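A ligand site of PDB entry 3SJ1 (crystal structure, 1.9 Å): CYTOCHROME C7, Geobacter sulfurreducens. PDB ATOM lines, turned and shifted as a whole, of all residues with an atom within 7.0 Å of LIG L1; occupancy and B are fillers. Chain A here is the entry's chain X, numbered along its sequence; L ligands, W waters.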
ATOM      1  N   ALA A   1      17.108  13.371 -37.913  1.00  0.00           N
ATOM      2  CA  ALA A   1      18.084  12.434 -38.519  1.00  0.00           C
ATOM      3  C   ALA A   1      17.892  11.042 -37.965  1.00  0.00           C
ATOM      4  O   ALA A   1      17.276  10.843 -36.925  1.00  0.00           O
ATOM      5  CB  ALA A   1      19.498  12.893 -38.264  1.00  0.00           C
ATOM      6  N   ASP A   2      18.451  10.076 -38.674  1.00  0.00           N
ATOM      7  CA  ASP A   2      18.265   8.691 -38.341  1.00  0.00           C
ATOM      8  C   ASP A   2      19.329   8.238 -37.374  1.00  0.00           C
ATOM      9  O   ASP A   2      20.424   8.795 -37.304  1.00  0.00           O
ATOM     10  CB  ASP A   2      18.378   7.863 -39.621  1.00  0.00           C
ATOM     11  CG  ASP A   2      17.228   8.099 -40.529  1.00  0.00           C
ATOM     12  OD1 ASP A   2      16.079   7.871 -40.061  1.00  0.00           O
ATOM     13  OD2 ASP A   2      17.368   8.532 -41.706  1.00  0.00           O
ATOM     14  N   ASP A   3      19.008   7.188 -36.639  1.00  0.00           N
ATOM     15  CA  ASP A   3      20.006   6.486 -35.842  1.00  0.00           C
ATOM     16  C   ASP A   3      21.053   5.871 -36.741  1.00  0.00           C
ATOM     17  O   ASP A   3      20.850   5.696 -37.950  1.00  0.00           O
ATOM     18  CB  ASP A   3      19.364   5.397 -34.994  1.00  0.00           C
ATOM     19  CG  ASP A   3      18.533   5.981 -33.858  1.00  0.00           C
ATOM     20  OD1 ASP A   3      18.703   7.181 -33.537  1.00  0.00           O
ATOM     21  OD2 ASP A   3      17.689   5.320 -33.245  1.00  0.00           O
ATOM     22  N   ILE A   4      22.209   5.597 -36.165  1.00  0.00           N
ATOM     23  CA  ILE A   4      23.252   4.974 -36.937  1.00  0.00           C
ATOM     24  C   ILE A   4      23.672   3.650 -36.323  1.00  0.00           C
ATOM     25  O   ILE A   4      23.441   3.400 -35.155  1.00  0.00           O
ATOM     26  CB  ILE A   4      24.465   5.939 -37.114  1.00  0.00           C
ATOM     27  CG1 ILE A   4      25.612   5.631 -36.148  1.00  0.00           C
ATOM     28  CG2 ILE A   4      24.054   7.386 -36.925  1.00  0.00           C
ATOM     29  CD1 ILE A   4      26.950   6.031 -36.684  1.00  0.00           C
ATOM     30  N   PHE A  15      23.119   2.711 -32.302  1.00  0.00           N
ATOM     31  CA  PHE A  15      23.245   3.860 -31.434  1.00  0.00           C
ATOM     32  C   PHE A  15      21.901   4.613 -31.490  1.00  0.00           C
ATOM     33  O   PHE A  15      21.603   5.245 -32.504  1.00  0.00           O
ATOM     34  CB  PHE A  15      24.353   4.812 -31.876  1.00  0.00           C
ATOM     35  CG  PHE A  15      24.381   6.069 -31.058  1.00  0.00           C
ATOM     36  CD1 PHE A  15      24.803   6.025 -29.720  1.00  0.00           C
ATOM     37  CD2 PHE A  15      23.878   7.259 -31.562  1.00  0.00           C
ATOM     38  CE1 PHE A  15      24.786   7.145 -28.918  1.00  0.00           C
ATOM     39  CE2 PHE A  15      23.832   8.403 -30.759  1.00  0.00           C
ATOM     40  CZ  PHE A  15      24.287   8.347 -29.441  1.00  0.00           C
ATOM     41  N   PRO A  16      21.077   4.463 -30.458  1.00  0.00           N
ATOM     42  CA  PRO A  16      19.769   5.124 -30.400  1.00  0.00           C
ATOM     43  C   PRO A  16      19.847   6.524 -29.810  1.00  0.00           C
ATOM     44  O   PRO A  16      19.988   6.682 -28.604  1.00  0.00           O
ATOM     45  CB  PRO A  16      18.950   4.176 -29.510  1.00  0.00           C
ATOM     46  CG  PRO A  16      19.979   3.599 -28.565  1.00  0.00           C
ATOM     47  CD  PRO A  16      21.299   3.576 -29.299  1.00  0.00           C
ATOM     48  N   HIS A  17      19.727   7.537 -30.667  1.00  0.00           N
ATOM     49  CA  HIS A  17      19.951   8.910 -30.206  1.00  0.00           C
ATOM     50  C   HIS A  17      18.932   9.391 -29.169  1.00  0.00           C
ATOM     51  O   HIS A  17      19.323   9.972 -28.160  1.00  0.00           O
ATOM     52  CB  HIS A  17      20.003   9.910 -31.353  1.00  0.00           C
ATOM     53  CG  HIS A  17      20.434  11.284 -30.913  1.00  0.00           C
ATOM     54  ND1 HIS A  17      19.565  12.350 -30.845  1.00  0.00           N
ATOM     55  CD2 HIS A  17      21.627  11.731 -30.451  1.00  0.00           C
ATOM     56  CE1 HIS A  17      20.220  13.421 -30.430  1.00  0.00           C
ATOM     57  NE2 HIS A  17      21.468  13.071 -30.177  1.00  0.00           N
ATOM     58  N   LYS A  18      17.646   9.151 -29.424  1.00  0.00           N
ATOM     59  CA  LYS A  18      16.582   9.586 -28.524  1.00  0.00           C
ATOM     60  C   LYS A  18      16.875   9.232 -27.064  1.00  0.00           C
ATOM     61  O   LYS A  18      16.804  10.072 -26.185  1.00  0.00           O
ATOM     62  CB  LYS A  18      15.228   8.965 -28.908  1.00  0.00           C
ATOM     63  N   HIS A  20      19.652   8.639 -25.626  1.00  0.00           N
ATOM     64  CA  HIS A  20      20.803   9.396 -25.157  1.00  0.00           C
ATOM     65  C   HIS A  20      20.504  10.854 -24.862  1.00  0.00           C
ATOM     66  O   HIS A  20      20.953  11.368 -23.869  1.00  0.00           O
ATOM     67  CB  HIS A  20      21.986   9.239 -26.101  1.00  0.00           C
ATOM     68  CG  HIS A  20      22.548   7.867 -26.047  1.00  0.00           C
ATOM     69  ND1 HIS A  20      22.080   6.847 -26.839  1.00  0.00           N
ATOM     70  CD2 HIS A  20      23.509   7.320 -25.263  1.00  0.00           C
ATOM     71  CE1 HIS A  20      22.742   5.734 -26.570  1.00  0.00           C
ATOM     72  NE2 HIS A  20      23.605   5.983 -25.603  1.00  0.00           N
ATOM     73  N   GLN A  21      19.763  11.498 -25.740  1.00  0.00           N
ATOM     74  CA  GLN A  21      19.313  12.864 -25.506  1.00  0.00           C
ATOM     75  C   GLN A  21      18.528  12.959 -24.176  1.00  0.00           C
ATOM     76  O   GLN A  21      18.710  13.894 -23.389  1.00  0.00           O
ATOM     77  CB  GLN A  21      18.434  13.268 -26.687  1.00  0.00           C
ATOM     78  CG  GLN A  21      18.312  14.729 -26.967  1.00  0.00           C
ATOM     79  CD  GLN A  21      17.823  14.991 -28.399  1.00  0.00           C
ATOM     80  OE1 GLN A  21      17.179  14.003 -28.986  1.00  0.00           O
ATOM     81  NE2 GLN A  21      18.045  16.070 -28.954  1.00  0.00           N
ATOM     82  N   LYS A  22      17.689  11.959 -23.938  1.00  0.00           N
ATOM     83  CA  LYS A  22      16.881  11.879 -22.714  1.00  0.00           C
ATOM     84  C   LYS A  22      17.708  11.588 -21.448  1.00  0.00           C
ATOM     85  O   LYS A  22      17.565  12.278 -20.393  1.00  0.00           O
ATOM     86  CB  LYS A  22      15.771  10.829 -22.911  1.00  0.00           C
ATOM     87  CG  LYS A  22      14.732  10.790 -21.801  1.00  0.00           C
ATOM     88  N   ALA A  23      18.587  10.596 -21.538  1.00  0.00           N
ATOM     89  CA  ALA A  23      19.343  10.097 -20.399  1.00  0.00           C
ATOM     90  C   ALA A  23      20.573  10.912 -20.090  1.00  0.00           C
ATOM     91  O   ALA A  23      21.030  10.913 -18.960  1.00  0.00           O
ATOM     92  CB  ALA A  23      19.719   8.619 -20.593  1.00  0.00           C
ATOM     93  N   VAL A  24      21.103  11.617 -21.093  1.00  0.00           N
ATOM     94  CA  VAL A  24      22.315  12.413 -20.952  1.00  0.00           C
ATOM     95  C   VAL A  24      22.016  13.833 -21.429  1.00  0.00           C
ATOM     96  O   VAL A  24      22.439  14.270 -22.512  1.00  0.00           O
ATOM     97  CB  VAL A  24      23.519  11.779 -21.730  1.00  0.00           C
ATOM     98  CG1 VAL A  24      24.796  12.544 -21.450  1.00  0.00           C
ATOM     99  CG2 VAL A  24      23.681  10.279 -21.385  1.00  0.00           C
ATOM    100  N   PRO A  25      21.214  14.552 -20.635  1.00  0.00           N
ATOM    101  CA  PRO A  25      20.838  15.934 -20.972  1.00  0.00           C
ATOM    102  C   PRO A  25      22.001  16.920 -21.038  1.00  0.00           C
ATOM    103  O   PRO A  25      21.867  17.966 -21.651  1.00  0.00           O
ATOM    104  CB  PRO A  25      19.855  16.323 -19.852  1.00  0.00           C
ATOM    105  CG  PRO A  25      20.200  15.396 -18.725  1.00  0.00           C
ATOM    106  CD  PRO A  25      20.575  14.103 -19.386  1.00  0.00           C
ATOM    107  N   ASP A  26      23.125  16.587 -20.424  1.00  0.00           N
ATOM    108  CA  ASP A  26      24.366  17.289 -20.663  1.00  0.00           C
ATOM    109  C   ASP A  26      24.935  16.961 -22.069  1.00  0.00           C
ATOM    110  O   ASP A  26      25.774  16.070 -22.242  1.00  0.00           O
ATOM    111  CB  ASP A  26      25.383  16.940 -19.588  1.00  0.00           C
ATOM    112  CG  ASP A  26      26.595  17.835 -19.632  1.00  0.00           C
ATOM    113  OD1 ASP A  26      26.682  18.695 -20.541  1.00  0.00           O
ATOM    114  OD2 ASP A  26      27.541  17.740 -18.810  1.00  0.00           O
ATOM    115  N   CYS A  27      24.525  17.751 -23.049  1.00  0.00           N
ATOM    116  CA  CYS A  27      24.810  17.471 -24.471  1.00  0.00           C
ATOM    117  C   CYS A  27      26.277  17.538 -24.791  1.00  0.00           C
ATOM    118  O   CYS A  27      26.731  16.880 -25.729  1.00  0.00           O
ATOM    119  CB  CYS A  27      24.059  18.453 -25.359  1.00  0.00           C
ATOM    120  SG  CYS A  27      22.298  18.611 -24.981  1.00  0.00           S
ATOM    121  N   LYS A  28      27.040  18.334 -24.035  1.00  0.00           N
ATOM    122  CA  LYS A  28      28.457  18.504 -24.270  1.00  0.00           C
ATOM    123  C   LYS A  28      29.312  17.278 -23.906  1.00  0.00           C
ATOM    124  O   LYS A  28      30.506  17.243 -24.195  1.00  0.00           O
ATOM    125  CB  LYS A  28      28.979  19.733 -23.508  1.00  0.00           C
ATOM    126  CG  LYS A  28      28.537  21.062 -24.097  1.00  0.00           C
ATOM    127  CD  LYS A  28      29.348  22.209 -23.479  1.00  0.00           C
ATOM    128  CE  LYS A  28      30.694  22.319 -24.119  1.00  0.00           C
ATOM    129  NZ  LYS A  28      31.520  23.367 -23.471  1.00  0.00           N
ATOM    130  N   LYS A  29      28.705  16.264 -23.317  1.00  0.00           N
ATOM    131  CA  LYS A  29      29.372  14.974 -23.166  1.00  0.00           C
ATOM    132  C   LYS A  29      29.740  14.408 -24.545  1.00  0.00           C
ATOM    133  O   LYS A  29      30.681  13.731 -24.644  1.00  0.00           O
ATOM    134  CB  LYS A  29      28.548  13.961 -22.357  1.00  0.00           C
ATOM    135  CG  LYS A  29      28.495  14.177 -20.919  1.00  0.00           C
ATOM    136  CD  LYS A  29      29.717  13.739 -20.170  1.00  0.00           C
ATOM    137  CE  LYS A  29      29.631  14.073 -18.639  1.00  0.00           C
ATOM    138  NZ  LYS A  29      28.339  14.573 -18.170  1.00  0.00           N
ATOM    139  N   CYS A  30      28.955  14.716 -25.560  1.00  0.00           N
ATOM    140  CA  CYS A  30      29.194  14.281 -26.956  1.00  0.00           C
ATOM    141  C   CYS A  30      29.335  15.368 -28.021  1.00  0.00           C
ATOM    142  O   CYS A  30      30.053  15.171 -29.021  1.00  0.00           O
ATOM    143  CB  CYS A  30      28.032  13.408 -27.373  1.00  0.00           C
ATOM    144  SG  CYS A  30      27.970  11.874 -26.397  1.00  0.00           S
ATOM    145  N   HIS A  31      28.618  16.487 -27.840  1.00  0.00           N
ATOM    146  CA  HIS A  31      28.561  17.545 -28.831  1.00  0.00           C
ATOM    147  C   HIS A  31      29.523  18.704 -28.499  1.00  0.00           C
ATOM    148  O   HIS A  31      29.944  18.893 -27.347  1.00  0.00           O
ATOM    149  CB  HIS A  31      27.103  18.017 -29.023  1.00  0.00           C
ATOM    150  CG  HIS A  31      26.233  16.978 -29.676  1.00  0.00           C
ATOM    151  ND1 HIS A  31      26.582  16.369 -30.863  1.00  0.00           N
ATOM    152  CD2 HIS A  31      25.045  16.427 -29.310  1.00  0.00           C
ATOM    153  CE1 HIS A  31      25.654  15.488 -31.194  1.00  0.00           C
ATOM    154  NE2 HIS A  31      24.710  15.500 -30.280  1.00  0.00           N
ATOM    155  N   GLY A  50      34.001   6.236 -25.058  1.00  0.00           N
ATOM    156  CA  GLY A  50      33.118   6.444 -26.179  1.00  0.00           C
ATOM    157  C   GLY A  50      31.752   5.789 -26.079  1.00  0.00           C
ATOM    158  O   GLY A  50      30.786   6.341 -26.597  1.00  0.00           O
ATOM    159  N   CYS A  54      31.121   5.042 -20.480  1.00  0.00           N
ATOM    160  CA  CYS A  54      30.048   5.889 -19.959  1.00  0.00           C
ATOM    161  C   CYS A  54      28.932   5.085 -19.317  1.00  0.00           C
ATOM    162  O   CYS A  54      28.444   5.447 -18.253  1.00  0.00           O
ATOM    163  CB  CYS A  54      29.498   6.827 -21.022  1.00  0.00           C
ATOM    164  SG  CYS A  54      28.177   7.893 -20.330  1.00  0.00           S
HETATM  165 FE1  LIG L   1      23.073  14.330 -30.146  1.00  0.00          FE
HETATM  166  C1  LIG L   1      22.610  13.831 -33.482  1.00  0.00           C
HETATM  167  C2  LIG L   1      21.357  17.277 -30.349  1.00  0.00           C
HETATM  168  C3  LIG L   1      22.895  14.436 -26.711  1.00  0.00           C
HETATM  169  C4  LIG L   1      25.427  11.931 -29.978  1.00  0.00           C
HETATM  170  N1  LIG L   1      22.239  15.400 -31.625  1.00  0.00           N
HETATM  171  C5  LIG L   1      22.032  14.954 -32.919  1.00  0.00           C
HETATM  172  C6  LIG L   1      21.087  15.818 -33.567  1.00  0.00           C
HETATM  173  C7  LIG L   1      20.723  16.756 -32.714  1.00  0.00           C
HETATM  174  C8  LIG L   1      21.458  16.533 -31.488  1.00  0.00           C
HETATM  175  C9  LIG L   1      19.744  17.920 -33.000  1.00  0.00           C
HETATM  176  C10 LIG L   1      20.529  15.618 -34.983  1.00  0.00           C
HETATM  177  C11 LIG L   1      19.442  14.553 -34.746  1.00  0.00           C
HETATM  178  C12 LIG L   1      18.230  14.660 -35.633  1.00  0.00           C
HETATM  179  O1  LIG L   1      18.120  15.603 -36.491  1.00  0.00           O
HETATM  180  O2  LIG L   1      17.331  13.766 -35.484  1.00  0.00           O
HETATM  181  N2  LIG L   1      22.231  15.589 -28.772  1.00  0.00           N
HETATM  182  C13 LIG L   1      21.593  16.780 -29.070  1.00  0.00           C
HETATM  183  C14 LIG L   1      21.203  17.410 -27.822  1.00  0.00           C
HETATM  184  C15 LIG L   1      21.625  16.603 -26.807  1.00  0.00           C
HETATM  185  C16 LIG L   1      22.298  15.463 -27.401  1.00  0.00           C
HETATM  186  C17 LIG L   1      20.434  18.750 -27.772  1.00  0.00           C
HETATM  187  C18 LIG L   1      21.490  16.749 -25.276  1.00  0.00           C
HETATM  188  C19 LIG L   1      20.235  16.856 -24.769  1.00  0.00           C
HETATM  189  N3  LIG L   1      23.986  13.374 -28.640  1.00  0.00           N
HETATM  190  C20 LIG L   1      23.802  13.554 -27.264  1.00  0.00           C
HETATM  191  C21 LIG L   1      24.658  12.647 -26.556  1.00  0.00           C
HETATM  192  C22 LIG L   1      25.344  11.947 -27.465  1.00  0.00           C
HETATM  193  C23 LIG L   1      24.947  12.402 -28.785  1.00  0.00           C
HETATM  194  C24 LIG L   1      24.742  12.591 -25.023  1.00  0.00           C
HETATM  195  C25 LIG L   1      26.418  10.849 -27.214  1.00  0.00           C
HETATM  196  C26 LIG L   1      26.124   9.873 -26.315  1.00  0.00           C
HETATM  197  N4  LIG L   1      23.923  13.113 -31.545  1.00  0.00           N
HETATM  198  C27 LIG L   1      24.878  12.182 -31.219  1.00  0.00           C
HETATM  199  C28 LIG L   1      25.179  11.447 -32.422  1.00  0.00           C
HETATM  200  C29 LIG L   1      24.300  11.987 -33.529  1.00  0.00           C
HETATM  201  C30 LIG L   1      23.540  13.044 -32.877  1.00  0.00           C
HETATM  202  C31 LIG L   1      26.194  10.314 -32.537  1.00  0.00           C
HETATM  203  C32 LIG L   1      24.240  11.533 -34.994  1.00  0.00           C
HETATM  204  C33 LIG L   1      23.698  10.107 -35.084  1.00  0.00           C
HETATM  205  C34 LIG L   1      22.269   9.930 -34.641  1.00  0.00           C
HETATM  206  O3  LIG L   1      21.437  10.823 -34.860  1.00  0.00           O
HETATM  207  O4  LIG L   1      21.971   8.841 -34.082  1.00  0.00           O
HETATM  208 FE1  LG2 L   2      24.687   4.711 -24.454  1.00  0.00          FE
HETATM  209  C1  LG2 L   2      21.693   3.624 -23.275  1.00  0.00           C
HETATM  210  C2  LG2 L   2      24.520   2.334 -26.953  1.00  0.00           C
HETATM  211  C3  LG2 L   2      27.490   6.011 -25.912  1.00  0.00           C
HETATM  212  C4  LG2 L   2      25.055   6.823 -21.857  1.00  0.00           C
HETATM  213  N1  LG2 L   2      23.363   3.245 -25.006  1.00  0.00           N
HETATM  214  C5  LG2 L   2      22.174   3.000 -24.393  1.00  0.00           C
HETATM  215  C6  LG2 L   2      21.485   1.954 -25.140  1.00  0.00           C
HETATM  216  C7  LG2 L   2      22.268   1.587 -26.160  1.00  0.00           C
HETATM  217  C8  LG2 L   2      23.454   2.396 -26.102  1.00  0.00           C
HETATM  218  C9  LG2 L   2      21.944   0.495 -27.214  1.00  0.00           C
HETATM  219  C10 LG2 L   2      20.113   1.356 -24.749  1.00  0.00           C
HETATM  220  C11 LG2 L   2      18.995   2.317 -25.048  1.00  0.00           C
HETATM  221  C12 LG2 L   2      17.665   1.741 -24.639  1.00  0.00           C
HETATM  222  O1  LG2 L   2      17.623   0.862 -23.747  1.00  0.00           O
HETATM  223  O2  LG2 L   2      16.653   2.155 -25.227  1.00  0.00           O
HETATM  224  N2  LG2 L   2      25.774   4.264 -26.116  1.00  0.00           N
HETATM  225  C13 LG2 L   2      25.580   3.221 -26.968  1.00  0.00           C
HETATM  226  C14 LG2 L   2      26.639   3.217 -27.957  1.00  0.00           C
HETATM  227  C15 LG2 L   2      27.451   4.233 -27.680  1.00  0.00           C
HETATM  228  C16 LG2 L   2      26.915   4.926 -26.523  1.00  0.00           C
HETATM  229  C17 LG2 L   2      26.752   2.166 -29.081  1.00  0.00           C
HETATM  230  C18 LG2 L   2      28.710   4.658 -28.456  1.00  0.00           C
HETATM  231  C19 LG2 L   2      28.582   4.706 -29.813  1.00  0.00           C
HETATM  232  N3  LG2 L   2      26.046   6.144 -23.967  1.00  0.00           N
HETATM  233  C20 LG2 L   2      27.133   6.535 -24.702  1.00  0.00           C
HETATM  234  C21 LG2 L   2      27.783   7.632 -24.009  1.00  0.00           C
HETATM  235  C22 LG2 L   2      27.097   7.851 -22.878  1.00  0.00           C
HETATM  236  C23 LG2 L   2      25.987   6.930 -22.852  1.00  0.00           C
HETATM  237  C24 LG2 L   2      29.063   8.359 -24.478  1.00  0.00           C
HETATM  238  C25 LG2 L   2      27.380   8.922 -21.788  1.00  0.00           C
HETATM  239  C26 LG2 L   2      28.094  10.001 -22.130  1.00  0.00           C
HETATM  240  N4  LG2 L   2      23.579   5.151 -22.875  1.00  0.00           N
HETATM  241  C27 LG2 L   2      23.941   6.045 -21.865  1.00  0.00           C
HETATM  242  C28 LG2 L   2      22.988   6.017 -20.786  1.00  0.00           C
HETATM  243  C29 LG2 L   2      21.945   5.020 -21.222  1.00  0.00           C
HETATM  244  C30 LG2 L   2      22.377   4.545 -22.518  1.00  0.00           C
HETATM  245  C31 LG2 L   2      23.015   6.831 -19.457  1.00  0.00           C
HETATM  246  C32 LG2 L   2      20.666   4.578 -20.497  1.00  0.00           C
HETATM  247  C33 LG2 L   2      19.502   5.081 -21.327  1.00  0.00           C
HETATM  248  C34 LG2 L   2      18.197   4.427 -20.957  1.00  0.00           C
HETATM  249  O3  LG2 L   2      18.167   3.206 -20.684  1.00  0.00           O
HETATM  250  O4  LG2 L   2      17.179   5.175 -20.936  1.00  0.00           O
HETATM  251  C1  LG3 L   3      32.155   7.084 -36.207  1.00  0.00           C
HETATM  252  C2  LG3 L   3      31.178   6.731 -35.065  1.00  0.00           C
HETATM  253  C3  LG3 L   3      30.026   7.765 -34.987  1.00  0.00           C
HETATM  254  C4  LG3 L   3      30.549   9.200 -34.743  1.00  0.00           C
HETATM  255  C5  LG3 L   3      31.622   9.529 -35.798  1.00  0.00           C
HETATM  256  C6  LG3 L   3      32.739   8.465 -35.881  1.00  0.00           C
HETATM  257  C7  LG3 L   3      28.989   7.301 -33.928  1.00  0.00           C
HETATM  258  C8  LG3 L   3      29.574   7.436 -32.507  1.00  0.00           C
HETATM  259  C9  LG3 L   3      30.049   8.879 -32.259  1.00  0.00           C
HETATM  260  C10 LG3 L   3      31.100   9.326 -33.313  1.00  0.00           C
HETATM  261  C11 LG3 L   3      30.671   9.013 -30.877  1.00  0.00           C
HETATM  262  C12 LG3 L   3      31.072  10.469 -30.559  1.00  0.00           C
HETATM  263  C13 LG3 L   3      32.162  10.897 -31.558  1.00  0.00           C
HETATM  264  C14 LG3 L   3      31.689  10.728 -33.015  1.00  0.00           C
HETATM  265  C15 LG3 L   3      29.745   8.611 -29.720  1.00  0.00           C
HETATM  266  C16 LG3 L   3      30.450   9.279 -28.525  1.00  0.00           C
HETATM  267  C17 LG3 L   3      31.533  10.210 -29.116  1.00  0.00           C
HETATM  268  C18 LG3 L   3      29.383  10.161 -34.974  1.00  0.00           C
HETATM  269  C19 LG3 L   3      31.717  11.458 -28.209  1.00  0.00           C
HETATM  270  O1  LG3 L   3      33.350  10.115 -31.423  1.00  0.00           O
HETATM  271  O2  LG3 L   3      33.228   6.113 -36.268  1.00  0.00           O
HETATM  272  C20 LG3 L   3      29.850  11.408 -30.662  1.00  0.00           C
HETATM  273  C21 LG3 L   3      31.917  11.059 -26.734  1.00  0.00           C
HETATM  274  C22 LG3 L   3      33.095  10.112 -26.486  1.00  0.00           C
HETATM  275  C23 LG3 L   3      34.377  10.888 -26.225  1.00  0.00           C
HETATM  276  O3  LG3 L   3      34.450  11.694 -25.295  1.00  0.00           O
HETATM  277  O4  LG3 L   3      35.361  10.716 -26.932  1.00  0.00           O
HETATM  278  C24 LG3 L   3      32.840  12.340 -28.725  1.00  0.00           C
HETATM  279  O   HOH W   1      18.961  10.192 -34.568  1.00  0.00           O
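The side-chain sulfur (SG) of Cys 30 is bonded to a carbon (C25) of LIG L1 (2.0 Å). A ring nitrogen (NE2) of His 31 is bound to an iron atom (FE1) of LIG L1. A ring nitrogen (NE2) of His 20 is bound to an iron atom (FE1) of LG2 L2 (2.0 Å). The backbone NH (N) of Ala 1 lies within hydrogen-bond range of an oxygen (O2) of LIG L1, 2.5 Å away. SG of Cys 27 is covalently linked to C18 of LIG L1. NE2 of His 17 binds FE1 of LIG L1 (2.0 Å). The side-chain sulfur (SG) of Cys 54 is covalently linked to a carbon (C25) of LG2 L2 (2.0 Å).
The backbone NH of His 17 sits at hydrogen-bond distance from the side-chain carboxylate of Asp 3, at 3.1 Å. ND1 of His 17 lies close to OE1 of Gln 21 (3.4 Å). N of Phe 15 lies within hydrogen-bond range of O of Ile 4, 3.0 Å away. O of Pro 16 is in hydrogen-bond range of ND1 of His 20, at 2.7 Å.
An oxygen (O3) of LIG L1 sits close to the backbone carbonyl oxygen of Asp 2 (3.3 Å). Merely in contact with LIG L1: Asp 3 (3.5 Å), Ile 4 (3.3 Å), Phe 15 (3.5 Å), His 20 (3.8 Å), Gln 21 (3.6 Å), Val 24 (3.6 Å) and Pro 25 (3.7 Å). Hydrophobic or aromatic side chains that line LIG L1: Ala 1, Ile 4, Phe 15, His 17, His 20, Val 24 and His 31. Within 4 Å of LIG L1: Ala 1, Asp 2, Asp 3, Ile 4, Phe 15, His 17, His 20, Gln 21, Val 24, Pro 25, Cys 27, Cys 30 and His 31.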
